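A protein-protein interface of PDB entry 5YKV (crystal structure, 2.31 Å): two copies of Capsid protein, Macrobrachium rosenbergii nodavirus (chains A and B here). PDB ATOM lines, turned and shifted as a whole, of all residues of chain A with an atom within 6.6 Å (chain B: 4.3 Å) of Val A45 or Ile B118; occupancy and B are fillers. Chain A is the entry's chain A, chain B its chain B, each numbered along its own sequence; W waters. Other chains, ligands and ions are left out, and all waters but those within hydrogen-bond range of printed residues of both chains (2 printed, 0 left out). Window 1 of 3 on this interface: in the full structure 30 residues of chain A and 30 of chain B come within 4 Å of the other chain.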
ATOM      1  N   TYR A  11      -1.442   4.844 -10.395  1.00  0.00           N
ATOM      2  CA  TYR A  11      -2.451   5.335 -11.277  1.00  0.00           C
ATOM      3  C   TYR A  11      -3.693   4.452 -11.152  1.00  0.00           C
ATOM      4  O   TYR A  11      -3.586   3.296 -10.933  1.00  0.00           O
ATOM      5  CB  TYR A  11      -1.943   5.361 -12.709  1.00  0.00           C
ATOM      6  CG  TYR A  11      -0.729   6.206 -12.982  1.00  0.00           C
ATOM      7  CD1 TYR A  11      -0.850   7.497 -13.458  1.00  0.00           C
ATOM      8  CD2 TYR A  11       0.544   5.662 -12.910  1.00  0.00           C
ATOM      9  CE1 TYR A  11       0.266   8.265 -13.744  1.00  0.00           C
ATOM     10  CE2 TYR A  11       1.669   6.414 -13.199  1.00  0.00           C
ATOM     11  CZ  TYR A  11       1.531   7.719 -13.619  1.00  0.00           C
ATOM     12  OH  TYR A  11       2.636   8.454 -13.923  1.00  0.00           O
ATOM     13  N   TRP A  19     -19.375   7.460 -24.919  1.00  0.00           N
ATOM     14  CA  TRP A  19     -19.804   8.732 -25.373  1.00  0.00           C
ATOM     15  C   TRP A  19     -21.218   8.594 -25.929  1.00  0.00           C
ATOM     16  O   TRP A  19     -21.504   7.705 -26.675  1.00  0.00           O
ATOM     17  CB  TRP A  19     -18.862   9.276 -26.449  1.00  0.00           C
ATOM     18  CG  TRP A  19     -17.479   9.583 -25.973  1.00  0.00           C
ATOM     19  CD1 TRP A  19     -16.318   8.977 -26.362  1.00  0.00           C
ATOM     20  CD2 TRP A  19     -17.097  10.650 -25.092  1.00  0.00           C
ATOM     21  NE1 TRP A  19     -15.244   9.587 -25.765  1.00  0.00           N
ATOM     22  CE2 TRP A  19     -15.689  10.626 -24.998  1.00  0.00           C
ATOM     23  CE3 TRP A  19     -17.806  11.572 -24.338  1.00  0.00           C
ATOM     24  CZ2 TRP A  19     -14.982  11.483 -24.160  1.00  0.00           C
ATOM     25  CZ3 TRP A  19     -17.112  12.444 -23.524  1.00  0.00           C
ATOM     26  CH2 TRP A  19     -15.725  12.391 -23.430  1.00  0.00           C
ATOM     27  N   ILE A  43      -6.695  12.665 -16.860  1.00  0.00           N
ATOM     28  CA  ILE A  43      -6.417  12.576 -18.281  1.00  0.00           C
ATOM     29  C   ILE A  43      -7.438  11.603 -18.856  1.00  0.00           C
ATOM     30  O   ILE A  43      -7.621  10.530 -18.300  1.00  0.00           O
ATOM     31  CB  ILE A  43      -4.991  12.079 -18.504  1.00  0.00           C
ATOM     32  CG1 ILE A  43      -4.107  13.171 -19.071  1.00  0.00           C
ATOM     33  CG2 ILE A  43      -4.987  10.891 -19.433  1.00  0.00           C
ATOM     34  CD1 ILE A  43      -3.834  12.989 -20.546  1.00  0.00           C
ATOM     35  N   ILE A  44      -8.068  11.972 -19.969  1.00  0.00           N
ATOM     36  CA  ILE A  44      -8.997  11.105 -20.623  1.00  0.00           C
ATOM     37  C   ILE A  44      -8.418  10.781 -21.990  1.00  0.00           C
ATOM     38  O   ILE A  44      -7.870  11.645 -22.666  1.00  0.00           O
ATOM     39  CB  ILE A  44     -10.402  11.715 -20.676  1.00  0.00           C
ATOM     40  CG1 ILE A  44     -11.418  10.786 -21.342  1.00  0.00           C
ATOM     41  CG2 ILE A  44     -10.355  13.078 -21.327  1.00  0.00           C
ATOM     42  CD1 ILE A  44     -12.856  11.224 -21.108  1.00  0.00           C
ATOM     43  N   VAL A  45      -8.455   9.486 -22.297  1.00  0.00           N
ATOM     44  CA  VAL A  45      -7.914   8.930 -23.504  1.00  0.00           C
ATOM     45  C   VAL A  45      -9.003   8.098 -24.163  1.00  0.00           C
ATOM     46  O   VAL A  45      -9.849   7.508 -23.496  1.00  0.00           O
ATOM     47  CB  VAL A  45      -6.658   8.069 -23.255  1.00  0.00           C
ATOM     48  CG1 VAL A  45      -5.516   8.888 -22.706  1.00  0.00           C
ATOM     49  CG2 VAL A  45      -6.936   6.871 -22.356  1.00  0.00           C
ATOM     50  N   PRO A  46      -9.021   8.020 -25.496  1.00  0.00           N
ATOM     51  CA  PRO A  46      -9.920   7.091 -26.172  1.00  0.00           C
ATOM     52  C   PRO A  46      -9.384   5.640 -26.152  1.00  0.00           C
ATOM     53  O   PRO A  46      -8.153   5.378 -26.027  1.00  0.00           O
ATOM     54  CB  PRO A  46      -9.922   7.655 -27.591  1.00  0.00           C
ATOM     55  CG  PRO A  46      -8.501   8.155 -27.765  1.00  0.00           C
ATOM     56  CD  PRO A  46      -8.180   8.782 -26.424  1.00  0.00           C
ATOM     57  N   TYR A  47     -10.316   4.691 -26.225  1.00  0.00           N
ATOM     58  CA  TYR A  47      -9.990   3.355 -26.510  1.00  0.00           C
ATOM     59  C   TYR A  47     -11.066   2.843 -27.469  1.00  0.00           C
ATOM     60  O   TYR A  47     -12.041   3.538 -27.730  1.00  0.00           O
ATOM     61  CB  TYR A  47      -9.822   2.552 -25.216  1.00  0.00           C
ATOM     62  CG  TYR A  47     -11.093   2.028 -24.602  1.00  0.00           C
ATOM     63  CD1 TYR A  47     -11.586   0.759 -24.896  1.00  0.00           C
ATOM     64  CD2 TYR A  47     -11.809   2.805 -23.711  1.00  0.00           C
ATOM     65  CE1 TYR A  47     -12.752   0.270 -24.305  1.00  0.00           C
ATOM     66  CE2 TYR A  47     -12.965   2.334 -23.117  1.00  0.00           C
ATOM     67  CZ  TYR A  47     -13.438   1.066 -23.411  1.00  0.00           C
ATOM     68  OH  TYR A  47     -14.612   0.673 -22.833  1.00  0.00           O
ATOM     69  N   ILE A  72      -9.643  14.759 -28.815  1.00  0.00           N
ATOM     70  CA  ILE A  72      -9.775  13.325 -29.085  1.00  0.00           C
ATOM     71  C   ILE A  72     -10.539  13.136 -30.400  1.00  0.00           C
ATOM     72  O   ILE A  72     -11.527  13.870 -30.654  1.00  0.00           O
ATOM     73  CB  ILE A  72     -10.502  12.606 -27.934  1.00  0.00           C
ATOM     74  CG1 ILE A  72      -9.646  12.567 -26.663  1.00  0.00           C
ATOM     75  CG2 ILE A  72     -10.936  11.202 -28.336  1.00  0.00           C
ATOM     76  CD1 ILE A  72     -10.386  12.031 -25.450  1.00  0.00           C
ATOM     77  N   TYR A  74     -12.082   9.959 -33.122  1.00  0.00           N
ATOM     78  CA  TYR A  74     -12.470   8.628 -33.458  1.00  0.00           C
ATOM     79  C   TYR A  74     -12.837   8.550 -34.942  1.00  0.00           C
ATOM     80  O   TYR A  74     -13.505   9.436 -35.456  1.00  0.00           O
ATOM     81  CB  TYR A  74     -13.692   8.215 -32.635  1.00  0.00           C
ATOM     82  CG  TYR A  74     -13.517   8.200 -31.143  1.00  0.00           C
ATOM     83  CD1 TYR A  74     -12.990   7.106 -30.496  1.00  0.00           C
ATOM     84  CD2 TYR A  74     -13.892   9.281 -30.376  1.00  0.00           C
ATOM     85  CE1 TYR A  74     -12.819   7.081 -29.120  1.00  0.00           C
ATOM     86  CE2 TYR A  74     -13.743   9.268 -28.999  1.00  0.00           C
ATOM     87  CZ  TYR A  74     -13.233   8.155 -28.359  1.00  0.00           C
ATOM     88  OH  TYR A  74     -13.081   8.140 -27.000  1.00  0.00           O
ATOM     89  N   CYS A  82      -8.171   6.321 -33.256  1.00  0.00           N
ATOM     90  CA  CYS A  82      -8.472   6.249 -31.835  1.00  0.00           C
ATOM     91  C   CYS A  82      -7.364   7.021 -31.117  1.00  0.00           C
ATOM     92  O   CYS A  82      -6.472   6.418 -30.555  1.00  0.00           O
ATOM     93  CB  CYS A  82      -8.529   4.799 -31.361  1.00  0.00           C
ATOM     94  SG  CYS A  82      -9.029   4.552 -29.626  1.00  0.00           S
ATOM     95  N   GLY A  84      -5.452  11.041 -29.664  1.00  0.00           N
ATOM     96  CA  GLY A  84      -5.561  12.256 -28.879  1.00  0.00           C
ATOM     97  C   GLY A  84      -5.753  11.954 -27.402  1.00  0.00           C
ATOM     98  O   GLY A  84      -5.682  10.804 -26.952  1.00  0.00           O
ATOM     99  N   TYR A  85      -5.972  13.012 -26.632  1.00  0.00           N
ATOM    100  CA  TYR A  85      -6.167  12.943 -25.190  1.00  0.00           C
ATOM    101  C   TYR A  85      -6.617  14.318 -24.692  1.00  0.00           C
ATOM    102  O   TYR A  85      -6.388  15.369 -25.355  1.00  0.00           O
ATOM    103  CB  TYR A  85      -4.893  12.538 -24.442  1.00  0.00           C
ATOM    104  CG  TYR A  85      -3.773  13.541 -24.517  1.00  0.00           C
ATOM    105  CD1 TYR A  85      -2.777  13.417 -25.470  1.00  0.00           C
ATOM    106  CD2 TYR A  85      -3.716  14.631 -23.669  1.00  0.00           C
ATOM    107  CE1 TYR A  85      -1.751  14.343 -25.579  1.00  0.00           C
ATOM    108  CE2 TYR A  85      -2.678  15.562 -23.746  1.00  0.00           C
ATOM    109  CZ  TYR A  85      -1.694  15.415 -24.705  1.00  0.00           C
ATOM    110  OH  TYR A  85      -0.657  16.289 -24.791  1.00  0.00           O
ATOM    111  N   ILE A  86      -7.264  14.317 -23.526  1.00  0.00           N
ATOM    112  CA  ILE A  86      -7.593  15.560 -22.888  1.00  0.00           C
ATOM    113  C   ILE A  86      -7.170  15.489 -21.426  1.00  0.00           C
ATOM    114  O   ILE A  86      -7.635  14.636 -20.689  1.00  0.00           O
ATOM    115  CB  ILE A  86      -9.085  15.917 -23.018  1.00  0.00           C
ATOM    116  CG1 ILE A  86      -9.546  15.909 -24.478  1.00  0.00           C
ATOM    117  CG2 ILE A  86      -9.341  17.262 -22.363  1.00  0.00           C
ATOM    118  CD1 ILE A  86     -11.042  16.037 -24.673  1.00  0.00           C
ATOM    119  N   GLN A 114     -15.766   5.106 -27.177  1.00  0.00           N
ATOM    120  CA  GLN A 114     -15.465   4.647 -25.823  1.00  0.00           C
ATOM    121  C   GLN A 114     -14.250   5.392 -25.274  1.00  0.00           C
ATOM    122  O   GLN A 114     -13.363   5.746 -26.047  1.00  0.00           O
ATOM    123  CB  GLN A 114     -15.221   3.139 -25.853  1.00  0.00           C
ATOM    124  CG  GLN A 114     -16.381   2.318 -26.414  1.00  0.00           C
ATOM    125  CD  GLN A 114     -15.865   1.043 -27.035  1.00  0.00           C
ATOM    126  OE1 GLN A 114     -15.098   1.073 -28.002  1.00  0.00           O
ATOM    127  NE2 GLN A 114     -16.275  -0.090 -26.474  1.00  0.00           N
ATOM    128  N   TYR A 115     -14.208   5.587 -23.947  1.00  0.00           N
ATOM    129  CA  TYR A 115     -13.128   6.391 -23.333  1.00  0.00           C
ATOM    130  C   TYR A 115     -12.653   5.775 -22.022  1.00  0.00           C
ATOM    131  O   TYR A 115     -13.390   5.056 -21.373  1.00  0.00           O
ATOM    132  CB  TYR A 115     -13.547   7.843 -23.056  1.00  0.00           C
ATOM    133  CG  TYR A 115     -14.653   8.023 -22.043  1.00  0.00           C
ATOM    134  CD1 TYR A 115     -14.393   8.025 -20.674  1.00  0.00           C
ATOM    135  CD2 TYR A 115     -15.958   8.251 -22.453  1.00  0.00           C
ATOM    136  CE1 TYR A 115     -15.410   8.186 -19.749  1.00  0.00           C
ATOM    137  CE2 TYR A 115     -16.984   8.412 -21.539  1.00  0.00           C
ATOM    138  CZ  TYR A 115     -16.709   8.387 -20.186  1.00  0.00           C
ATOM    139  OH  TYR A 115     -17.713   8.545 -19.292  1.00  0.00           O
ATOM    140  N   ARG A 116     -11.449   6.196 -21.619  1.00  0.00           N
ATOM    141  CA  ARG A 116     -10.835   5.776 -20.392  1.00  0.00           C
ATOM    142  C   ARG A 116     -10.309   6.999 -19.640  1.00  0.00           C
ATOM    143  O   ARG A 116      -9.542   7.782 -20.199  1.00  0.00           O
ATOM    144  CB  ARG A 116      -9.685   4.801 -20.665  1.00  0.00           C
ATOM    145  CG  ARG A 116      -8.987   4.301 -19.408  1.00  0.00           C
ATOM    146  CD  ARG A 116      -7.910   3.257 -19.663  1.00  0.00           C
ATOM    147  NE  ARG A 116      -8.350   2.199 -20.560  1.00  0.00           N
ATOM    148  CZ  ARG A 116      -8.953   1.084 -20.178  1.00  0.00           C
ATOM    149  NH1 ARG A 116      -9.183   0.862 -18.891  1.00  0.00           N
ATOM    150  NH2 ARG A 116      -9.301   0.197 -21.095  1.00  0.00           N
ATOM    151  N   ILE A 117     -10.652   7.078 -18.351  1.00  0.00           N
ATOM    152  CA  ILE A 117     -10.186   8.149 -17.485  1.00  0.00           C
ATOM    153  C   ILE A 117      -9.073   7.641 -16.578  1.00  0.00           C
ATOM    154  O   ILE A 117      -9.183   6.588 -15.955  1.00  0.00           O
ATOM    155  CB  ILE A 117     -11.337   8.780 -16.685  1.00  0.00           C
ATOM    156  CG1 ILE A 117     -12.364   9.403 -17.634  1.00  0.00           C
ATOM    157  CG2 ILE A 117     -10.778   9.810 -15.691  1.00  0.00           C
ATOM    158  CD1 ILE A 117     -13.650   9.865 -16.993  1.00  0.00           C
ATOM    159  N   ILE A 118      -7.960   8.388 -16.578  1.00  0.00           N
ATOM    160  CA  ILE A 118      -6.791   8.068 -15.771  1.00  0.00           C
ATOM    161  C   ILE A 118      -6.576   9.154 -14.708  1.00  0.00           C
ATOM    162  O   ILE A 118      -6.481  10.376 -15.020  1.00  0.00           O
ATOM    163  CB  ILE A 118      -5.544   7.895 -16.658  1.00  0.00           C
ATOM    164  CG1 ILE A 118      -5.736   6.769 -17.675  1.00  0.00           C
ATOM    165  CG2 ILE A 118      -4.304   7.680 -15.796  1.00  0.00           C
ATOM    166  CD1 ILE A 118      -4.819   6.862 -18.882  1.00  0.00           C
ATOM    167  N   TYR B  11      -0.073  15.968 -16.180  1.00  0.00           N
ATOM    168  CA  TYR B  11       0.250  14.774 -16.911  1.00  0.00           C
ATOM    169  C   TYR B  11       0.982  15.184 -18.185  1.00  0.00           C
ATOM    170  O   TYR B  11       0.626  16.161 -18.786  1.00  0.00           O
ATOM    171  CB  TYR B  11      -0.996  13.966 -17.262  1.00  0.00           C
ATOM    172  CG  TYR B  11      -1.845  13.569 -16.088  1.00  0.00           C
ATOM    173  CD1 TYR B  11      -1.676  12.356 -15.442  1.00  0.00           C
ATOM    174  CD2 TYR B  11      -2.859  14.398 -15.649  1.00  0.00           C
ATOM    175  CE1 TYR B  11      -2.471  11.997 -14.361  1.00  0.00           C
ATOM    176  CE2 TYR B  11      -3.666  14.054 -14.579  1.00  0.00           C
ATOM    177  CZ  TYR B  11      -3.471  12.856 -13.921  1.00  0.00           C
ATOM    178  OH  TYR B  11      -4.285  12.561 -12.864  1.00  0.00           O
ATOM    179  N   ASN B  12       2.041  14.453 -18.528  1.00  0.00           N
ATOM    180  CA  ASN B  12       2.693  14.552 -19.819  1.00  0.00           C
ATOM    181  C   ASN B  12       2.295  13.294 -20.593  1.00  0.00           C
ATOM    182  O   ASN B  12       2.495  12.161 -20.101  1.00  0.00           O
ATOM    183  CB  ASN B  12       4.211  14.700 -19.691  1.00  0.00           C
ATOM    184  CG  ASN B  12       4.893  14.836 -21.037  1.00  0.00           C
ATOM    185  OD1 ASN B  12       4.922  13.911 -21.850  1.00  0.00           O
ATOM    186  ND2 ASN B  12       5.439  16.005 -21.298  1.00  0.00           N
ATOM    187  N   ALA B  13       1.695  13.501 -21.767  1.00  0.00           N
ATOM    188  CA  ALA B  13       1.145  12.418 -22.550  1.00  0.00           C
ATOM    189  C   ALA B  13       1.588  12.505 -24.016  1.00  0.00           C
ATOM    190  O   ALA B  13       0.910  11.962 -24.902  1.00  0.00           O
ATOM    191  CB  ALA B  13      -0.355  12.454 -22.440  1.00  0.00           C
ATOM    192  N   PHE B  42       4.812   5.014 -14.891  1.00  0.00           N
ATOM    193  CA  PHE B  42       4.037   5.377 -16.036  1.00  0.00           C
ATOM    194  C   PHE B  42       2.811   4.487 -16.189  1.00  0.00           C
ATOM    195  O   PHE B  42       2.732   3.398 -15.644  1.00  0.00           O
ATOM    196  CB  PHE B  42       4.874   5.181 -17.284  1.00  0.00           C
ATOM    197  CG  PHE B  42       6.159   5.951 -17.313  1.00  0.00           C
ATOM    198  CD1 PHE B  42       6.207   7.228 -17.836  1.00  0.00           C
ATOM    199  CD2 PHE B  42       7.331   5.372 -16.867  1.00  0.00           C
ATOM    200  CE1 PHE B  42       7.402   7.922 -17.904  1.00  0.00           C
ATOM    201  CE2 PHE B  42       8.519   6.082 -16.909  1.00  0.00           C
ATOM    202  CZ  PHE B  42       8.555   7.351 -17.433  1.00  0.00           C
ATOM    203  N   ILE B  43       1.875   4.981 -16.995  1.00  0.00           N
ATOM    204  CA  ILE B  43       0.812   4.176 -17.641  1.00  0.00           C
ATOM    205  C   ILE B  43       1.020   4.279 -19.146  1.00  0.00           C
ATOM    206  O   ILE B  43       1.108   5.386 -19.678  1.00  0.00           O
ATOM    207  CB  ILE B  43      -0.594   4.679 -17.285  1.00  0.00           C
ATOM    208  CG1 ILE B  43      -0.842   4.570 -15.794  1.00  0.00           C
ATOM    209  CG2 ILE B  43      -1.669   3.918 -18.052  1.00  0.00           C
ATOM    210  CD1 ILE B  43      -1.303   3.206 -15.384  1.00  0.00           C
ATOM    211  N   ARG B 116       1.006   5.296 -26.513  1.00  0.00           N
ATOM    212  CA  ARG B 116       1.209   6.560 -25.891  1.00  0.00           C
ATOM    213  C   ARG B 116       1.625   6.321 -24.445  1.00  0.00           C
ATOM    214  O   ARG B 116       1.016   5.543 -23.735  1.00  0.00           O
ATOM    215  CB  ARG B 116      -0.071   7.378 -25.975  1.00  0.00           C
ATOM    216  CG  ARG B 116       0.003   8.712 -25.247  1.00  0.00           C
ATOM    217  CD  ARG B 116      -1.306   9.471 -25.336  1.00  0.00           C
ATOM    218  NE  ARG B 116      -1.769   9.567 -26.708  1.00  0.00           N
ATOM    219  CZ  ARG B 116      -1.357  10.443 -27.592  1.00  0.00           C
ATOM    220  NH1 ARG B 116      -0.466  11.354 -27.259  1.00  0.00           N
ATOM    221  NH2 ARG B 116      -1.901  10.435 -28.792  1.00  0.00           N
ATOM    222  N   ILE B 117       2.645   7.042 -23.996  1.00  0.00           N
ATOM    223  CA  ILE B 117       3.088   6.912 -22.605  1.00  0.00           C
ATOM    224  C   ILE B 117       2.643   8.125 -21.780  1.00  0.00           C
ATOM    225  O   ILE B 117       2.885   9.266 -22.155  1.00  0.00           O
ATOM    226  CB  ILE B 117       4.603   6.714 -22.577  1.00  0.00           C
ATOM    227  CG1 ILE B 117       4.932   5.268 -22.960  1.00  0.00           C
ATOM    228  CG2 ILE B 117       5.159   7.114 -21.209  1.00  0.00           C
ATOM    229  CD1 ILE B 117       6.389   5.009 -23.170  1.00  0.00           C
ATOM    230  N   ILE B 118       2.006   7.843 -20.638  1.00  0.00           N
ATOM    231  CA  ILE B 118       1.497   8.857 -19.738  1.00  0.00           C
ATOM    232  C   ILE B 118       2.310   8.854 -18.424  1.00  0.00           C
ATOM    233  O   ILE B 118       2.456   7.826 -17.780  1.00  0.00           O
ATOM    234  CB  ILE B 118       0.009   8.599 -19.502  1.00  0.00           C
ATOM    235  CG1 ILE B 118      -0.746   8.609 -20.831  1.00  0.00           C
ATOM    236  CG2 ILE B 118      -0.572   9.600 -18.521  1.00  0.00           C
ATOM    237  CD1 ILE B 118      -2.222   8.465 -20.684  1.00  0.00           C
ATOM    238  N   ARG B 119       2.789  10.046 -18.031  1.00  0.00           N
ATOM    239  CA  ARG B 119       3.664  10.297 -16.868  1.00  0.00           C
ATOM    240  C   ARG B 119       3.056  11.432 -16.019  1.00  0.00           C
ATOM    241  O   ARG B 119       2.867  12.541 -16.496  1.00  0.00           O
ATOM    242  CB  ARG B 119       5.040  10.714 -17.404  1.00  0.00           C
ATOM    243  CG  ARG B 119       6.096  11.086 -16.374  1.00  0.00           C
ATOM    244  CD  ARG B 119       7.317  11.748 -17.026  1.00  0.00           C
ATOM    245  NE  ARG B 119       8.203  12.317 -16.017  1.00  0.00           N
ATOM    246  CZ  ARG B 119       8.891  13.450 -16.140  1.00  0.00           C
ATOM    247  NH1 ARG B 119       9.525  13.961 -15.092  1.00  0.00           N
ATOM    248  NH2 ARG B 119       8.945  14.068 -17.307  1.00  0.00           N
HETATM  249  O   HOH W   1       0.895  16.112 -22.443  1.00  0.00           O
HETATM  250  O   HOH W   2      -4.299   8.733 -27.637  1.00  0.00           O
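Of the printed residues of chain B, Ile A43 touches Tyr B11 (3.7 Å), Ala B13 (3.997 Å) and Ile B118 (3.9 Å). Val A45 touches just one residue of chain B: Ile B118 (3.9 Å). Of the printed residues of chain B, Tyr A85 touches Ala B13 (3.6 Å) and Arg B116 (3.6 Å). Of the printed residues of chain A, Tyr B11 touches Ile A43 and Ile A118. Printed residues of chain A within 4 Å of Ile B43: Tyr A11. Ile B118 touches four residues of chain A. Of the printed residues of chain A, Arg B119 touches Tyr A11 (3.6 Å). The nearest printed residue of chain B that does not touch Val A45 is Arg B116 (5.0 Å). The nearest residue of chain A that does not touch Ile B118 is Tyr A85 (6.2 Å).
The backbone NH (N) of Ile A118 is in hydrogen-bond range of the backbone carbonyl oxygen (O) of Ile A43 (2.8 Å). The backbone NH (N) of Arg A116 lies within hydrogen-bond range of the backbone carbonyl oxygen (O) of Val A45, 2.8 Å away. The backbone NH of Asn B12 is in hydrogen-bond range of the backbone carbonyl oxygen of Arg B119, 2.9 Å away. The backbone carbonyl oxygen of Ala B13 is in hydrogen-bond range of the guanidinium group of Arg B116 (2.8 Å). O of Ile B43 lies within hydrogen-bond range of N of Ile B118.
Water W2 bridges the backbone carbonyl oxygen of Gly A84 and the guanidinium group of Arg B116. Water W1 lies within hydrogen-bond range of the backbone NH (N) of Ala B13 and the side-chain hydroxyl (OH) of Tyr A85.
Among the printed residues, merely in contact across the chains: Tyr A11 with Ile B43, Ile A118 with Ile B118, Tyr A85 with Arg B116, Tyr A11 with Arg B119, Tyr A85 with Ala B13, Ile A43 with Tyr B11, Gly A84 with Arg B116, Tyr A11 with Phe B42, Ile A118 with Tyr B11, Ile A43 with Ile B118, Val A45 with Ile B118, Tyr A11 with Ile B118 and Ile A43 with Ala B13.
Hydrophobic or aromatic side chains of chain A that line the printed part of chain B: Tyr A11, Ile A43, Val A45, Tyr A85 and Ile A118. Hydrophobic or aromatic side chains of chain B within 4 Å of the printed part of chain A: Tyr B11, Ala B13, Ile B43 and Ile B118. Among the printed residues, no Asp or Glu carboxylate lies within 4 Å of a Lys or Arg side-chain nitrogen of the other chain.
Tyr A11 touches Ile B43, and with the chains exchanged Ile A43 touches Tyr B11. Tyr A11 touches Ile B118, and with the chains exchanged Ile A118 touches Tyr B11. Ile A43 touches Ile B118, but with the chains exchanged Ile A118 does not touch Ile B43 (4.4 Å). Ile B118 touches its own counterpart, Ile A118. Positions printed for both chains: 11, 43, 116, 117 and 118. Of the 13 pairs that touch across the chains among the printed residues, 5 have their exchanged pair printed and touching as well.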
